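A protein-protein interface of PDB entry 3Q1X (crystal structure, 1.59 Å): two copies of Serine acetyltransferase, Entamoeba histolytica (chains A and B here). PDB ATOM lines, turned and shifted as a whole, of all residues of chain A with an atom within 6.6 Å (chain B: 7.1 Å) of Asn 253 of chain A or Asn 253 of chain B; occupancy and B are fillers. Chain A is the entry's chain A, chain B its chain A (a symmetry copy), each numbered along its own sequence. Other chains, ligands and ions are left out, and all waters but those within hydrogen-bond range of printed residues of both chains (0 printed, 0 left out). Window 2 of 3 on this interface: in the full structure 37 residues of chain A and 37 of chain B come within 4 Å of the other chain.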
ATOM      1  N   SER A 201      22.432  -5.957  26.083  1.00  0.00           N
ATOM      2  CA  SER A 201      21.880  -7.288  26.337  1.00  0.00           C
ATOM      3  C   SER A 201      22.850  -8.322  26.916  1.00  0.00           C
ATOM      4  O   SER A 201      22.597  -9.533  26.824  1.00  0.00           O
ATOM      5  CB  SER A 201      21.239  -7.828  25.050  1.00  0.00           C
ATOM      6  OG  SER A 201      20.011  -7.175  24.794  1.00  0.00           O
ATOM      7  N   GLY A 233      30.388  -9.398  23.835  1.00  0.00           N
ATOM      8  CA  GLY A 233      29.562  -9.017  22.697  1.00  0.00           C
ATOM      9  C   GLY A 233      28.076  -9.039  22.967  1.00  0.00           C
ATOM     10  O   GLY A 233      27.624  -9.610  23.964  1.00  0.00           O
ATOM     11  N   THR A 234      27.331  -8.406  22.065  1.00  0.00           N
ATOM     12  CA  THR A 234      25.886  -8.252  22.170  1.00  0.00           C
ATOM     13  C   THR A 234      25.154  -9.564  22.439  1.00  0.00           C
ATOM     14  O   THR A 234      25.323 -10.538  21.704  1.00  0.00           O
ATOM     15  CB  THR A 234      25.292  -7.652  20.882  1.00  0.00           C
ATOM     16  OG1 THR A 234      26.125  -6.580  20.408  1.00  0.00           O
ATOM     17  CG2 THR A 234      23.895  -7.144  21.158  1.00  0.00           C
ATOM     18  N   GLY A 235      24.339  -9.573  23.492  1.00  0.00           N
ATOM     19  CA  GLY A 235      23.466 -10.707  23.789  1.00  0.00           C
ATOM     20  C   GLY A 235      24.102 -11.854  24.555  1.00  0.00           C
ATOM     21  O   GLY A 235      23.421 -12.826  24.898  1.00  0.00           O
ATOM     22  N   ALA A 236      25.399 -11.746  24.830  1.00  0.00           N
ATOM     23  CA  ALA A 236      26.116 -12.808  25.539  1.00  0.00           C
ATOM     24  C   ALA A 236      25.578 -12.977  26.958  1.00  0.00           C
ATOM     25  O   ALA A 236      25.365 -11.989  27.670  1.00  0.00           O
ATOM     26  CB  ALA A 236      27.615 -12.535  25.544  1.00  0.00           C
ATOM     27  N   LYS A 237      25.325 -14.229  27.345  1.00  0.00           N
ATOM     28  CA  LYS A 237      24.811 -14.555  28.676  1.00  0.00           C
ATOM     29  C   LYS A 237      25.852 -15.363  29.437  1.00  0.00           C
ATOM     30  O   LYS A 237      26.026 -16.562  29.193  1.00  0.00           O
ATOM     31  CB  LYS A 237      23.477 -15.324  28.609  1.00  0.00           C
ATOM     32  CG  LYS A 237      22.356 -14.675  27.769  1.00  0.00           C
ATOM     33  CD  LYS A 237      22.133 -13.212  28.142  1.00  0.00           C
ATOM     34  CE  LYS A 237      20.949 -12.594  27.383  1.00  0.00           C
ATOM     35  NZ  LYS A 237      21.036 -12.697  25.901  1.00  0.00           N
ATOM     36  N   GLY A 251      31.816 -13.555  21.739  1.00  0.00           N
ATOM     37  CA  GLY A 251      30.980 -13.263  20.569  1.00  0.00           C
ATOM     38  C   GLY A 251      29.506 -13.061  20.868  1.00  0.00           C
ATOM     39  O   GLY A 251      29.035 -13.336  21.980  1.00  0.00           O
ATOM     40  N   ALA A 252      28.772 -12.586  19.863  1.00  0.00           N
ATOM     41  CA  ALA A 252      27.354 -12.249  20.025  1.00  0.00           C
ATOM     42  C   ALA A 252      26.488 -13.460  20.399  1.00  0.00           C
ATOM     43  O   ALA A 252      26.736 -14.581  19.952  1.00  0.00           O
ATOM     44  CB  ALA A 252      26.818 -11.563  18.773  1.00  0.00           C
ATOM     45  N   ASN A 253      25.485 -13.217  21.241  1.00  0.00           N
ATOM     46  CA  ASN A 253      24.510 -14.232  21.655  1.00  0.00           C
ATOM     47  C   ASN A 253      25.081 -15.490  22.323  1.00  0.00           C
ATOM     48  O   ASN A 253      24.392 -16.504  22.426  1.00  0.00           O
ATOM     49  CB  ASN A 253      23.596 -14.613  20.479  1.00  0.00           C
ATOM     50  CG  ASN A 253      22.510 -13.582  20.221  1.00  0.00           C
ATOM     51  OD1 ASN A 253      22.423 -12.566  20.912  1.00  0.00           O
ATOM     52  ND2 ASN A 253      21.673 -13.843  19.222  1.00  0.00           N
ATOM     53  N   CYS A 254      26.328 -15.422  22.784  1.00  0.00           N
ATOM     54  CA  CYS A 254      26.976 -16.582  23.394  1.00  0.00           C
ATOM     55  C   CYS A 254      26.421 -16.928  24.771  1.00  0.00           C
ATOM     56  O   CYS A 254      26.088 -16.057  25.565  1.00  0.00           O
ATOM     57  CB  CYS A 254      28.494 -16.401  23.455  1.00  0.00           C
ATOM     58  SG  CYS A 254      29.342 -16.849  21.919  1.00  0.00           S
ATOM     59  N   TRP A 255      26.335 -18.225  25.031  1.00  0.00           N
ATOM     60  CA  TRP A 255      25.789 -18.759  26.259  1.00  0.00           C
ATOM     61  C   TRP A 255      26.944 -19.419  27.019  1.00  0.00           C
ATOM     62  O   TRP A 255      27.379 -20.520  26.677  1.00  0.00           O
ATOM     63  CB  TRP A 255      24.652 -19.720  25.878  1.00  0.00           C
ATOM     64  CG  TRP A 255      24.150 -20.706  26.884  1.00  0.00           C
ATOM     65  CD1 TRP A 255      23.662 -21.958  26.610  1.00  0.00           C
ATOM     66  CD2 TRP A 255      24.047 -20.542  28.302  1.00  0.00           C
ATOM     67  NE1 TRP A 255      23.272 -22.580  27.766  1.00  0.00           N
ATOM     68  CE2 TRP A 255      23.502 -21.738  28.821  1.00  0.00           C
ATOM     69  CE3 TRP A 255      24.370 -19.509  29.187  1.00  0.00           C
ATOM     70  CZ2 TRP A 255      23.268 -21.925  30.180  1.00  0.00           C
ATOM     71  CZ3 TRP A 255      24.146 -19.703  30.535  1.00  0.00           C
ATOM     72  CH2 TRP A 255      23.595 -20.900  31.020  1.00  0.00           C
ATOM     73  N   SER B 201      15.089 -10.196  29.055  1.00  0.00           N
ATOM     74  CA  SER B 201      15.133 -10.502  27.625  1.00  0.00           C
ATOM     75  C   SER B 201      14.340 -11.730  27.171  1.00  0.00           C
ATOM     76  O   SER B 201      14.602 -12.275  26.088  1.00  0.00           O
ATOM     77  CB  SER B 201      16.597 -10.624  27.176  1.00  0.00           C
ATOM     78  OG  SER B 201      17.204  -9.348  27.102  1.00  0.00           O
ATOM     79  N   GLY B 233      14.774 -18.891  31.172  1.00  0.00           N
ATOM     80  CA  GLY B 233      16.091 -18.290  31.323  1.00  0.00           C
ATOM     81  C   GLY B 233      16.340 -17.095  30.434  1.00  0.00           C
ATOM     82  O   GLY B 233      15.598 -16.856  29.477  1.00  0.00           O
ATOM     83  N   THR B 234      17.391 -16.352  30.770  1.00  0.00           N
ATOM     84  CA  THR B 234      17.768 -15.122  30.085  1.00  0.00           C
ATOM     85  C   THR B 234      17.858 -15.274  28.571  1.00  0.00           C
ATOM     86  O   THR B 234      18.563 -16.153  28.070  1.00  0.00           O
ATOM     87  CB  THR B 234      19.132 -14.604  30.576  1.00  0.00           C
ATOM     88  OG1 THR B 234      19.218 -14.720  32.007  1.00  0.00           O
ATOM     89  CG2 THR B 234      19.307 -13.162  30.158  1.00  0.00           C
ATOM     90  N   GLY B 235      17.144 -14.409  27.852  1.00  0.00           N
ATOM     91  CA  GLY B 235      17.244 -14.341  26.395  1.00  0.00           C
ATOM     92  C   GLY B 235      16.395 -15.335  25.623  1.00  0.00           C
ATOM     93  O   GLY B 235      16.374 -15.309  24.388  1.00  0.00           O
ATOM     94  N   ALA B 236      15.692 -16.208  26.341  1.00  0.00           N
ATOM     95  CA  ALA B 236      14.863 -17.229  25.694  1.00  0.00           C
ATOM     96  C   ALA B 236      13.725 -16.588  24.904  1.00  0.00           C
ATOM     97  O   ALA B 236      13.055 -15.673  25.398  1.00  0.00           O
ATOM     98  CB  ALA B 236      14.333 -18.221  26.721  1.00  0.00           C
ATOM     99  N   LYS B 237      13.539 -17.047  23.665  1.00  0.00           N
ATOM    100  CA  LYS B 237      12.487 -16.538  22.784  1.00  0.00           C
ATOM    101  C   LYS B 237      11.482 -17.645  22.503  1.00  0.00           C
ATOM    102  O   LYS B 237      11.740 -18.547  21.700  1.00  0.00           O
ATOM    103  CB  LYS B 237      13.056 -15.981  21.464  1.00  0.00           C
ATOM    104  CG  LYS B 237      14.174 -14.924  21.594  1.00  0.00           C
ATOM    105  CD  LYS B 237      13.791 -13.798  22.551  1.00  0.00           C
ATOM    106  CE  LYS B 237      14.857 -12.692  22.602  1.00  0.00           C
ATOM    107  NZ  LYS B 237      16.226 -13.162  22.946  1.00  0.00           N
ATOM    108  N   ILE B 250      13.734 -23.660  31.033  1.00  0.00           N
ATOM    109  CA  ILE B 250      14.228 -23.213  29.730  1.00  0.00           C
ATOM    110  C   ILE B 250      15.553 -22.474  29.880  1.00  0.00           C
ATOM    111  O   ILE B 250      15.651 -21.509  30.642  1.00  0.00           O
ATOM    112  CB  ILE B 250      13.194 -22.332  29.000  1.00  0.00           C
ATOM    113  CG1 ILE B 250      11.913 -23.133  28.739  1.00  0.00           C
ATOM    114  CG2 ILE B 250      13.766 -21.804  27.683  1.00  0.00           C
ATOM    115  CD1 ILE B 250      10.662 -22.285  28.637  1.00  0.00           C
ATOM    116  N   GLY B 251      16.566 -22.942  29.151  1.00  0.00           N
ATOM    117  CA  GLY B 251      17.924 -22.393  29.233  1.00  0.00           C
ATOM    118  C   GLY B 251      18.125 -21.068  28.522  1.00  0.00           C
ATOM    119  O   GLY B 251      17.259 -20.612  27.762  1.00  0.00           O
ATOM    120  N   ALA B 252      19.280 -20.451  28.763  1.00  0.00           N
ATOM    121  CA  ALA B 252      19.581 -19.120  28.226  1.00  0.00           C
ATOM    122  C   ALA B 252      19.611 -19.084  26.692  1.00  0.00           C
ATOM    123  O   ALA B 252      20.029 -20.044  26.043  1.00  0.00           O
ATOM    124  CB  ALA B 252      20.887 -18.588  28.809  1.00  0.00           C
ATOM    125  N   ASN B 253      19.140 -17.974  26.128  1.00  0.00           N
ATOM    126  CA  ASN B 253      19.156 -17.729  24.683  1.00  0.00           C
ATOM    127  C   ASN B 253      18.428 -18.762  23.811  1.00  0.00           C
ATOM    128  O   ASN B 253      18.638 -18.808  22.600  1.00  0.00           O
ATOM    129  CB  ASN B 253      20.595 -17.521  24.185  1.00  0.00           C
ATOM    130  CG  ASN B 253      21.126 -16.130  24.491  1.00  0.00           C
ATOM    131  OD1 ASN B 253      20.433 -15.301  25.082  1.00  0.00           O
ATOM    132  ND2 ASN B 253      22.365 -15.870  24.086  1.00  0.00           N
ATOM    133  N   CYS B 254      17.571 -19.577  24.421  1.00  0.00           N
ATOM    134  CA  CYS B 254      16.865 -20.626  23.685  1.00  0.00           C
ATOM    135  C   CYS B 254      15.786 -20.086  22.754  1.00  0.00           C
ATOM    136  O   CYS B 254      15.088 -19.129  23.069  1.00  0.00           O
ATOM    137  CB  CYS B 254      16.284 -21.675  24.634  1.00  0.00           C
ATOM    138  SG  CYS B 254      17.473 -22.948  25.128  1.00  0.00           S
ATOM    139  N   TRP B 255      15.666 -20.729  21.601  1.00  0.00           N
ATOM    140  CA  TRP B 255      14.737 -20.342  20.564  1.00  0.00           C
ATOM    141  C   TRP B 255      13.682 -21.450  20.463  1.00  0.00           C
ATOM    142  O   TRP B 255      13.938 -22.518  19.903  1.00  0.00           O
ATOM    143  CB  TRP B 255      15.548 -20.124  19.277  1.00  0.00           C
ATOM    144  CG  TRP B 255      14.845 -20.090  17.957  1.00  0.00           C
ATOM    145  CD1 TRP B 255      15.359 -20.520  16.760  1.00  0.00           C
ATOM    146  CD2 TRP B 255      13.537 -19.587  17.669  1.00  0.00           C
ATOM    147  NE1 TRP B 255      14.451 -20.323  15.755  1.00  0.00           N
ATOM    148  CE2 TRP B 255      13.322 -19.758  16.283  1.00  0.00           C
ATOM    149  CE3 TRP B 255      12.521 -19.019  18.444  1.00  0.00           C
ATOM    150  CZ2 TRP B 255      12.138 -19.376  15.657  1.00  0.00           C
ATOM    151  CZ3 TRP B 255      11.345 -18.652  17.822  1.00  0.00           C
ATOM    152  CH2 TRP B 255      11.164 -18.826  16.440  1.00  0.00           C
ATOM    153  N   ILE B 256      12.510 -21.197  21.043  1.00  0.00           N
ATOM    154  CA  ILE B 256      11.465 -22.223  21.169  1.00  0.00           C
ATOM    155  C   ILE B 256      10.250 -21.948  20.278  1.00  0.00           C
ATOM    156  O   ILE B 256       9.559 -20.935  20.420  1.00  0.00           O
ATOM    157  CB  ILE B 256      11.088 -22.489  22.653  1.00  0.00           C
ATOM    158  CG1 ILE B 256      12.293 -23.112  23.374  1.00  0.00           C
ATOM    159  CG2 ILE B 256       9.868 -23.404  22.754  1.00  0.00           C
ATOM    160  CD1 ILE B 256      12.147 -23.250  24.869  1.00  0.00           C
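CG2 of Thr 234 of chain B touches CE of Lys 237 of chain A (3.3 Å).
Ala 252 of chain B touches Trp 255 of chain A.
Of the 11 printed residues of chain A, 4 touch a printed residue of chain B.
Printed residues of chain A that touch a printed residue of chain B: Gly 235, Lys 237, Asn 253 and Trp 255.
Printed residues of chain B that touch a printed residue of chain A: Thr 234, Ala 252 and Asn 253.
Hydrophobic or aromatic side chains of chain B within 4 Å of the printed part of chain A: Ala 252.
Among the printed residues, 5 pairs touch across the chains.
Among the printed residues, no Asp or Glu carboxylate lies within 4 Å of a Lys or Arg side-chain nitrogen of the other chain.
Asn 253 of chain A touches just one residue of chain B: Asn 253.
Printed residues of chain A within 4 Å of Thr 234 of chain B: Lys 237 (3.3 Å).
Printed residues of chain B within 4 Å of Gly 235 of chain A: Asn 253 (3.3 Å).
Printed residues of chain B within 4 Å of Trp 255 of chain A: Ala 252.
Of the printed residues of chain A, Ala 252 of chain B touches Trp 255 (3.6 Å).
Printed residues of chain B within 4 Å of Lys 237 of chain A: Thr 234 (3.3 Å) and Asn 253 (2.8 Å).
Gly 233 of chain B touches none of the printed residues of chain A.
The nearest printed residue of chain A that does not touch Asn 253 of chain B is Cys 254 of chain A (4.01 Å).
The nearest printed residue of chain A that does not touch Thr 234 of chain B is Ser 201 of chain A (5.9 Å).
N of Lys 237 of chain A lies within hydrogen-bond range of O of Cys 254 of chain A, 2.7 Å away.
NZ of Lys 237 of chain A sits at hydrogen-bond distance from O of Gly 235 of chain A (2.6 Å).
The backbone carbonyl oxygen (O) of Thr 234 of chain B is in hydrogen-bond range of the backbone NH (N) of Asn 253 of chain B, 2.7 Å away.
O of Thr 234 of chain A is in hydrogen-bond range of N of Asn 253 of chain A (2.7 Å).
Gly 235 of chain A touches Asn 253 of chain B, but with the chains exchanged Asn 253 of chain A does not touch Gly 235 of chain B (7.5 Å).
Lys 237 of chain A touches Asn 253 of chain B, but with the chains exchanged Asn 253 of chain A does not touch Lys 237 of chain B (6.5 Å).
Asn 253 of chain B touches its own counterpart, Asn 253 of chain A.
Trp 255 of chain A touches Ala 252 of chain B, but with the chains exchanged Ala 252 of chain A does not touch Trp 255 of chain B (12.5 Å).
Positions printed for both chains: 201, 233, 234, 235, 236, 237, 251, 252, 253, 254 and 255.
The backbone carbonyl oxygen (O) of Gly 235 of chain A sits at hydrogen-bond distance from the side-chain amide nitrogen (ND2) of Asn 253 of chain B (3.3 Å).
The side-chain amino group of Lys 237 of chain A sits at hydrogen-bond distance from the side-chain amide oxygen of Asn 253 of chain B, 2.8 Å away.
The backbone carbonyl oxygen (O) of Asn 253 of chain A is in hydrogen-bond range of the side-chain amide nitrogen (ND2) of Asn 253 of chain B, 2.7 Å away.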
